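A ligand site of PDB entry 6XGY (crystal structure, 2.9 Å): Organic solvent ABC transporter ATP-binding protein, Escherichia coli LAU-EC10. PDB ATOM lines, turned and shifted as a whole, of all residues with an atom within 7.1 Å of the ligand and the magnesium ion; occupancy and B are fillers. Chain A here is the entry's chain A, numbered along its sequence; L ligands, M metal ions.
OE2 of Glu 170 is in salt-bridge range of NZ of Lys 47 (3.5 Å).
The backbone NH (N) of Glu 170 sits at hydrogen-bond distance from the backbone carbonyl oxygen (O) of Val 201 (2.8 Å).
The side-chain hydroxyl of Thr 48 lies close to the side-chain carboxylate of Asp 169, at 3.0 Å.
The side-chain amino group (NZ) of Lys 47 is in hydrogen-bond range of a ring nitrogen (NE2) of His 203 (3.1 Å).
The backbone NH (N) of Ile 23 sits at hydrogen-bond distance from the backbone carbonyl oxygen (O) of Phe 16, at 3.1 Å.
The magnesium ion is bound by O1 of the ligand and OG1 of Thr 48.
Residues that only touch the magnesium ion: Glu 170 (2.9 Å) and Asp 169 (3.1 Å).
The nearest printed residue that does not touch the magnesium ion is Lys 47 (4.7 Å).
Arg 18 touches the ligand.
CD1 of Ile 23 touches O8 of the ligand, at 3.4 Å.
N of Ile 45 touches O2 of the ligand, at 3.9 Å.
Hydrophobic or aromatic side chains within 4 Å of the ligand: Ile 23 and Ile 45.
An oxygen (O5) of the ligand sits at hydrogen-bond distance from the backbone NH (N) of Thr 49 (2.8 Å).
N of Thr 48 sits close to O1 of the ligand (3.4 Å).
N of Lys 47 sits at hydrogen-bond distance from O2 of the ligand, at 3.0 Å.
The side-chain hydroxyl (OG1) of Thr 49 is in hydrogen-bond range of an oxygen (O5) of the ligand (2.6 Å).
O of Gly 44 is in hydrogen-bond range of O9 of the ligand, at 3.0 Å.
The side-chain amino group (NZ) of Lys 47 is in salt-bridge range of an oxygen (O2) of the ligand.
N of Gly 46 lies within hydrogen-bond range of O6 of the ligand, 3.0 Å away.
The backbone NH of Gly 44 is in hydrogen-bond range of an oxygen (O3) of the ligand, at 2.9 Å.
The guanidinium group of Arg 21 sits at hydrogen-bond distance from an oxygen (O9) of the ligand.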
ATOM      1  N   PHE A  16      37.202  32.318  -9.543  1.00  0.00           N
ATOM      2  CA  PHE A  16      37.234  30.881  -9.761  1.00  0.00           C
ATOM      3  C   PHE A  16      36.789  30.571 -11.182  1.00  0.00           C
ATOM      4  O   PHE A  16      35.783  31.117 -11.644  1.00  0.00           O
ATOM      5  CB  PHE A  16      36.348  30.149  -8.747  1.00  0.00           C
ATOM      6  CG  PHE A  16      36.390  28.650  -8.859  1.00  0.00           C
ATOM      7  CD1 PHE A  16      37.546  27.953  -8.530  1.00  0.00           C
ATOM      8  CD2 PHE A  16      35.274  27.946  -9.262  1.00  0.00           C
ATOM      9  CE1 PHE A  16      37.586  26.573  -8.628  1.00  0.00           C
ATOM     10  CE2 PHE A  16      35.311  26.560  -9.350  1.00  0.00           C
ATOM     11  CZ  PHE A  16      36.466  25.880  -9.036  1.00  0.00           C
ATOM     12  N   ARG A  18      36.424  27.355 -14.233  1.00  0.00           N
ATOM     13  CA  ARG A  18      36.416  25.950 -14.623  1.00  0.00           C
ATOM     14  C   ARG A  18      36.442  25.867 -16.136  1.00  0.00           C
ATOM     15  O   ARG A  18      35.543  26.391 -16.806  1.00  0.00           O
ATOM     16  CB  ARG A  18      35.206  25.222 -14.067  1.00  0.00           C
ATOM     17  CG  ARG A  18      35.310  24.911 -12.586  1.00  0.00           C
ATOM     18  CD  ARG A  18      34.098  24.119 -12.153  1.00  0.00           C
ATOM     19  NE  ARG A  18      34.029  23.821 -10.729  1.00  0.00           N
ATOM     20  CZ  ARG A  18      34.714  22.855 -10.114  1.00  0.00           C
ATOM     21  NH1 ARG A  18      35.550  22.093 -10.811  1.00  0.00           N
ATOM     22  NH2 ARG A  18      34.567  22.660  -8.819  1.00  0.00           N
ATOM     23  N   GLY A  19      37.468  25.211 -16.669  1.00  0.00           N
ATOM     24  CA  GLY A  19      37.539  24.979 -18.115  1.00  0.00           C
ATOM     25  C   GLY A  19      37.598  26.300 -18.860  1.00  0.00           C
ATOM     26  O   GLY A  19      38.471  27.152 -18.614  1.00  0.00           O
ATOM     27  N   ASN A  20      36.658  26.496 -19.773  1.00  0.00           N
ATOM     28  CA  ASN A  20      36.622  27.689 -20.599  1.00  0.00           C
ATOM     29  C   ASN A  20      35.839  28.834 -19.958  1.00  0.00           C
ATOM     30  O   ASN A  20      36.021  29.990 -20.348  1.00  0.00           O
ATOM     31  CB  ASN A  20      36.000  27.377 -21.958  1.00  0.00           C
ATOM     32  CG  ASN A  20      34.612  26.776 -21.841  1.00  0.00           C
ATOM     33  OD1 ASN A  20      33.623  27.491 -21.702  1.00  0.00           O
ATOM     34  ND2 ASN A  20      34.533  25.448 -21.885  1.00  0.00           N
ATOM     35  N   ARG A  21      34.966  28.533 -18.993  1.00  0.00           N
ATOM     36  CA  ARG A  21      34.015  29.498 -18.482  1.00  0.00           C
ATOM     37  C   ARG A  21      34.372  29.913 -17.056  1.00  0.00           C
ATOM     38  O   ARG A  21      34.841  29.099 -16.262  1.00  0.00           O
ATOM     39  CB  ARG A  21      32.601  28.927 -18.513  1.00  0.00           C
ATOM     40  CG  ARG A  21      31.514  29.970 -18.314  1.00  0.00           C
ATOM     41  CD  ARG A  21      30.137  29.389 -18.570  1.00  0.00           C
ATOM     42  NE  ARG A  21      29.774  28.375 -17.581  1.00  0.00           N
ATOM     43  CZ  ARG A  21      29.208  28.642 -16.413  1.00  0.00           C
ATOM     44  NH1 ARG A  21      28.932  29.898 -16.076  1.00  0.00           N
ATOM     45  NH2 ARG A  21      28.907  27.656 -15.581  1.00  0.00           N
ATOM     46  N   ILE A  23      33.261  31.272 -13.353  1.00  0.00           N
ATOM     47  CA  ILE A  23      32.138  31.170 -12.440  1.00  0.00           C
ATOM     48  C   ILE A  23      32.062  32.361 -11.503  1.00  0.00           C
ATOM     49  O   ILE A  23      30.974  32.864 -11.217  1.00  0.00           O
ATOM     50  CB  ILE A  23      32.217  29.844 -11.652  1.00  0.00           C
ATOM     51  CG1 ILE A  23      32.027  28.674 -12.598  1.00  0.00           C
ATOM     52  CG2 ILE A  23      31.187  29.796 -10.538  1.00  0.00           C
ATOM     53  CD1 ILE A  23      32.854  27.496 -12.227  1.00  0.00           C
ATOM     54  N   PHE A  24      33.211  32.825 -11.013  1.00  0.00           N
ATOM     55  CA  PHE A  24      33.275  33.941 -10.071  1.00  0.00           C
ATOM     56  C   PHE A  24      34.282  34.962 -10.556  1.00  0.00           C
ATOM     57  O   PHE A  24      35.407  34.611 -10.940  1.00  0.00           O
ATOM     58  CB  PHE A  24      33.639  33.454  -8.673  1.00  0.00           C
ATOM     59  CG  PHE A  24      32.517  32.732  -7.963  1.00  0.00           C
ATOM     60  CD1 PHE A  24      31.237  33.245  -7.974  1.00  0.00           C
ATOM     61  CD2 PHE A  24      32.755  31.545  -7.294  1.00  0.00           C
ATOM     62  CE1 PHE A  24      30.207  32.585  -7.331  1.00  0.00           C
ATOM     63  CE2 PHE A  24      31.725  30.884  -6.651  1.00  0.00           C
ATOM     64  CZ  PHE A  24      30.455  31.406  -6.668  1.00  0.00           C
ATOM     65  N   GLY A  41      20.429  32.930  -5.479  1.00  0.00           N
ATOM     66  CA  GLY A  41      20.786  33.156  -6.860  1.00  0.00           C
ATOM     67  C   GLY A  41      20.241  32.086  -7.778  1.00  0.00           C
ATOM     68  O   GLY A  41      19.803  31.018  -7.328  1.00  0.00           O
ATOM     69  N   PRO A  42      20.262  32.353  -9.079  1.00  0.00           N
ATOM     70  CA  PRO A  42      19.741  31.363 -10.031  1.00  0.00           C
ATOM     71  C   PRO A  42      20.548  30.074 -10.004  1.00  0.00           C
ATOM     72  O   PRO A  42      21.690  30.025  -9.562  1.00  0.00           O
ATOM     73  CB  PRO A  42      19.867  32.071 -11.385  1.00  0.00           C
ATOM     74  CG  PRO A  42      19.935  33.529 -11.060  1.00  0.00           C
ATOM     75  CD  PRO A  42      20.658  33.599  -9.751  1.00  0.00           C
ATOM     76  N   SER A  43      19.908  29.003 -10.484  1.00  0.00           N
ATOM     77  CA  SER A  43      20.568  27.708 -10.552  1.00  0.00           C
ATOM     78  C   SER A  43      21.757  27.755 -11.505  1.00  0.00           C
ATOM     79  O   SER A  43      21.670  28.298 -12.603  1.00  0.00           O
ATOM     80  CB  SER A  43      19.581  26.631 -11.010  1.00  0.00           C
ATOM     81  OG  SER A  43      18.511  26.484 -10.089  1.00  0.00           O
ATOM     82  N   GLY A  44      22.875  27.187 -11.060  1.00  0.00           N
ATOM     83  CA  GLY A  44      24.081  27.146 -11.863  1.00  0.00           C
ATOM     84  C   GLY A  44      25.046  28.287 -11.658  1.00  0.00           C
ATOM     85  O   GLY A  44      26.040  28.383 -12.391  1.00  0.00           O
ATOM     86  N   ILE A  45      24.795  29.176 -10.689  1.00  0.00           N
ATOM     87  CA  ILE A  45      25.666  30.324 -10.496  1.00  0.00           C
ATOM     88  C   ILE A  45      26.957  29.935  -9.784  1.00  0.00           C
ATOM     89  O   ILE A  45      28.012  30.522 -10.053  1.00  0.00           O
ATOM     90  CB  ILE A  45      24.923  31.436  -9.741  1.00  0.00           C
ATOM     91  CG1 ILE A  45      25.835  32.651  -9.553  1.00  0.00           C
ATOM     92  CG2 ILE A  45      24.441  30.952  -8.387  1.00  0.00           C
ATOM     93  CD1 ILE A  45      25.273  33.895 -10.130  1.00  0.00           C
ATOM     94  N   GLY A  46      26.913  28.954  -8.897  1.00  0.00           N
ATOM     95  CA  GLY A  46      28.093  28.538  -8.172  1.00  0.00           C
ATOM     96  C   GLY A  46      27.923  28.582  -6.667  1.00  0.00           C
ATOM     97  O   GLY A  46      28.898  28.760  -5.933  1.00  0.00           O
ATOM     98  N   LYS A  47      26.684  28.438  -6.203  1.00  0.00           N
ATOM     99  CA  LYS A  47      26.416  28.447  -4.767  1.00  0.00           C
ATOM    100  C   LYS A  47      27.096  27.261  -4.083  1.00  0.00           C
ATOM    101  O   LYS A  47      27.802  27.435  -3.087  1.00  0.00           O
ATOM    102  CB  LYS A  47      24.907  28.431  -4.518  1.00  0.00           C
ATOM    103  CG  LYS A  47      24.193  29.689  -5.000  1.00  0.00           C
ATOM    104  CD  LYS A  47      22.678  29.535  -4.981  1.00  0.00           C
ATOM    105  CE  LYS A  47      22.139  29.056  -6.321  1.00  0.00           C
ATOM    106  NZ  LYS A  47      21.237  27.890  -6.211  1.00  0.00           N
ATOM    107  N   THR A  48      26.898  26.056  -4.617  1.00  0.00           N
ATOM    108  CA  THR A  48      27.599  24.886  -4.093  1.00  0.00           C
ATOM    109  C   THR A  48      29.110  25.041  -4.248  1.00  0.00           C
ATOM    110  O   THR A  48      29.876  24.625  -3.373  1.00  0.00           O
ATOM    111  CB  THR A  48      27.122  23.624  -4.803  1.00  0.00           C
ATOM    112  OG1 THR A  48      25.690  23.534  -4.716  1.00  0.00           O
ATOM    113  CG2 THR A  48      27.733  22.374  -4.164  1.00  0.00           C
ATOM    114  N   THR A  49      29.555  25.641  -5.356  1.00  0.00           N
ATOM    115  CA  THR A  49      30.975  25.915  -5.544  1.00  0.00           C
ATOM    116  C   THR A  49      31.497  26.838  -4.455  1.00  0.00           C
ATOM    117  O   THR A  49      32.553  26.598  -3.864  1.00  0.00           O
ATOM    118  CB  THR A  49      31.206  26.524  -6.920  1.00  0.00           C
ATOM    119  OG1 THR A  49      31.047  25.512  -7.927  1.00  0.00           O
ATOM    120  CG2 THR A  49      32.603  27.132  -7.009  1.00  0.00           C
ATOM    121  N   LEU A  50      30.749  27.910  -4.164  1.00  0.00           N
ATOM    122  CA  LEU A  50      31.168  28.855  -3.138  1.00  0.00           C
ATOM    123  C   LEU A  50      31.288  28.186  -1.770  1.00  0.00           C
ATOM    124  O   LEU A  50      32.160  28.571  -0.969  1.00  0.00           O
ATOM    125  CB  LEU A  50      30.176  30.015  -3.079  1.00  0.00           C
ATOM    126  CG  LEU A  50      30.397  31.094  -2.016  1.00  0.00           C
ATOM    127  CD1 LEU A  50      30.525  32.457  -2.660  1.00  0.00           C
ATOM    128  CD2 LEU A  50      29.266  31.074  -1.005  1.00  0.00           C
ATOM    129  N   LEU A  51      30.454  27.193  -1.481  1.00  0.00           N
ATOM    130  CA  LEU A  51      30.549  26.483  -0.207  1.00  0.00           C
ATOM    131  C   LEU A  51      31.805  25.631  -0.145  1.00  0.00           C
ATOM    132  O   LEU A  51      32.525  25.626   0.852  1.00  0.00           O
ATOM    133  CB  LEU A  51      29.303  25.637   0.024  1.00  0.00           C
ATOM    134  CG  LEU A  51      28.005  26.385   0.334  1.00  0.00           C
ATOM    135  CD1 LEU A  51      26.908  25.404   0.734  1.00  0.00           C
ATOM    136  CD2 LEU A  51      28.236  27.423   1.422  1.00  0.00           C
ATOM    137  N   ARG A  52      32.082  24.879  -1.222  1.00  0.00           N
ATOM    138  CA  ARG A  52      33.272  24.051  -1.261  1.00  0.00           C
ATOM    139  C   ARG A  52      34.556  24.861  -1.220  1.00  0.00           C
ATOM    140  O   ARG A  52      35.600  24.339  -0.820  1.00  0.00           O
ATOM    141  CB  ARG A  52      33.255  23.163  -2.500  1.00  0.00           C
ATOM    142  CG  ARG A  52      32.029  22.270  -2.586  1.00  0.00           C
ATOM    143  CD  ARG A  52      32.110  21.340  -3.785  1.00  0.00           C
ATOM    144  NE  ARG A  52      30.886  20.553  -3.941  1.00  0.00           N
ATOM    145  CZ  ARG A  52      30.643  19.762  -4.974  1.00  0.00           C
ATOM    146  NH1 ARG A  52      31.539  19.655  -5.951  1.00  0.00           N
ATOM    147  NH2 ARG A  52      29.509  19.087  -5.047  1.00  0.00           N
ATOM    148  N   ILE A  58      38.067  22.688  -2.776  1.00  0.00           N
ATOM    149  CA  ILE A  58      38.537  23.294  -4.013  1.00  0.00           C
ATOM    150  C   ILE A  58      39.159  24.631  -3.661  1.00  0.00           C
ATOM    151  O   ILE A  58      38.785  25.273  -2.679  1.00  0.00           O
ATOM    152  CB  ILE A  58      37.404  23.472  -5.068  1.00  0.00           C
ATOM    153  CG1 ILE A  58      36.282  24.359  -4.512  1.00  0.00           C
ATOM    154  CG2 ILE A  58      36.866  22.137  -5.542  1.00  0.00           C
ATOM    155  CD1 ILE A  58      35.152  24.578  -5.477  1.00  0.00           C
ATOM    156  N   ASP A 169      22.965  23.319   2.122  1.00  0.00           N
ATOM    157  CA  ASP A 169      22.914  23.453   0.662  1.00  0.00           C
ATOM    158  C   ASP A 169      21.501  23.098   0.198  1.00  0.00           C
ATOM    159  O   ASP A 169      21.173  21.920   0.042  1.00  0.00           O
ATOM    160  CB  ASP A 169      23.957  22.570   0.004  1.00  0.00           C
ATOM    161  CG  ASP A 169      24.314  23.030  -1.394  1.00  0.00           C
ATOM    162  OD1 ASP A 169      23.543  23.826  -1.973  1.00  0.00           O
ATOM    163  OD2 ASP A 169      25.372  22.615  -1.912  1.00  0.00           O
ATOM    164  N   GLU A 170      20.679  24.119  -0.026  1.00  0.00           N
ATOM    165  CA  GLU A 170      19.279  23.964  -0.409  1.00  0.00           C
ATOM    166  C   GLU A 170      18.568  22.938   0.462  1.00  0.00           C
ATOM    167  O   GLU A 170      18.063  21.924  -0.035  1.00  0.00           O
ATOM    168  CB  GLU A 170      19.165  23.600  -1.883  1.00  0.00           C
ATOM    169  CG  GLU A 170      19.726  24.660  -2.829  1.00  0.00           C
ATOM    170  CD  GLU A 170      19.509  24.321  -4.284  1.00  0.00           C
ATOM    171  OE1 GLU A 170      18.470  23.712  -4.614  1.00  0.00           O
ATOM    172  OE2 GLU A 170      20.385  24.669  -5.111  1.00  0.00           O
ATOM    173  N   VAL A 201      22.106  28.255   1.794  1.00  0.00           N
ATOM    174  CA  VAL A 201      21.779  28.432   0.380  1.00  0.00           C
ATOM    175  C   VAL A 201      20.374  27.882   0.157  1.00  0.00           C
ATOM    176  O   VAL A 201      20.058  26.779   0.609  1.00  0.00           O
ATOM    177  CB  VAL A 201      22.796  27.702  -0.510  1.00  0.00           C
ATOM    178  CG1 VAL A 201      22.364  27.740  -1.967  1.00  0.00           C
ATOM    179  CG2 VAL A 201      24.183  28.315  -0.349  1.00  0.00           C
ATOM    180  N   HIS A 203      16.462  28.458  -2.434  1.00  0.00           N
ATOM    181  CA  HIS A 203      15.590  29.170  -3.367  1.00  0.00           C
ATOM    182  C   HIS A 203      14.290  29.617  -2.723  1.00  0.00           C
ATOM    183  O   HIS A 203      13.592  30.466  -3.286  1.00  0.00           O
ATOM    184  CB  HIS A 203      15.268  28.295  -4.568  1.00  0.00           C
ATOM    185  CG  HIS A 203      16.434  28.058  -5.478  1.00  0.00           C
ATOM    186  ND1 HIS A 203      16.721  26.828  -6.015  1.00  0.00           N
ATOM    187  CD2 HIS A 203      17.384  28.910  -5.945  1.00  0.00           C
ATOM    188  CE1 HIS A 203      17.809  26.918  -6.770  1.00  0.00           C
ATOM    189  NE2 HIS A 203      18.227  28.169  -6.744  1.00  0.00           N
HETATM  190  P1  LIG L   1      24.693  25.754  -7.881  1.00  0.00           P
HETATM  191  O1  LIG L   1      24.753  24.682  -6.820  1.00  0.00           O
HETATM  192  O2  LIG L   1      24.269  27.120  -7.399  1.00  0.00           O
HETATM  193  O3  LIG L   1      24.014  25.324  -9.163  1.00  0.00           O
HETATM  194  P2  LIG L   1      27.275  24.918  -8.723  1.00  0.00           P
HETATM  195  O4  LIG L   1      26.581  23.572  -8.829  1.00  0.00           O
HETATM  196  O5  LIG L   1      28.511  25.060  -7.862  1.00  0.00           O
HETATM  197  O6  LIG L   1      26.211  26.048  -8.304  1.00  0.00           O
HETATM  198  O7  LIG L   1      27.633  25.427 -10.209  1.00  0.00           O
HETATM  199  C1  LIG L   1      28.954  25.415 -10.717  1.00  0.00           C
HETATM  200  C2  LIG L   1      28.901  25.828 -12.182  1.00  0.00           C
HETATM  201  O8  LIG L   1      30.137  25.464 -12.794  1.00  0.00           O
HETATM  202  C3  LIG L   1      27.789  25.097 -12.916  1.00  0.00           C
HETATM  203  O9  LIG L   1      27.117  25.993 -13.802  1.00  0.00           O
HETATM  204  C4  LIG L   1      28.480  24.028 -13.737  1.00  0.00           C
HETATM  205  O10 LIG L   1      27.950  24.014 -15.065  1.00  0.00           O
HETATM  206  C5  LIG L   1      29.949  24.430 -13.760  1.00  0.00           C
HETATM  207  N1  LIG L   1      30.799  23.281 -13.394  1.00  0.00           N
HETATM  208  C6  LIG L   1      30.744  22.607 -12.227  1.00  0.00           C
HETATM  209  N2  LIG L   1      31.661  21.601 -12.197  1.00  0.00           N
HETATM  210  C7  LIG L   1      32.308  21.618 -13.377  1.00  0.00           C
HETATM  211  C8  LIG L   1      33.399  20.828 -14.003  1.00  0.00           C
HETATM  212  N3  LIG L   1      33.984  19.793 -13.349  1.00  0.00           N
HETATM  213  N4  LIG L   1      33.796  21.176 -15.248  1.00  0.00           N
HETATM  214  C9  LIG L   1      33.225  22.206 -15.902  1.00  0.00           C
HETATM  215  N5  LIG L   1      32.236  22.963 -15.402  1.00  0.00           N
HETATM  216  C10 LIG L   1      31.745  22.720 -14.164  1.00  0.00           C
HETATM  217 MG    MG M   1      23.156  23.819  -5.033  1.00  0.00          MG
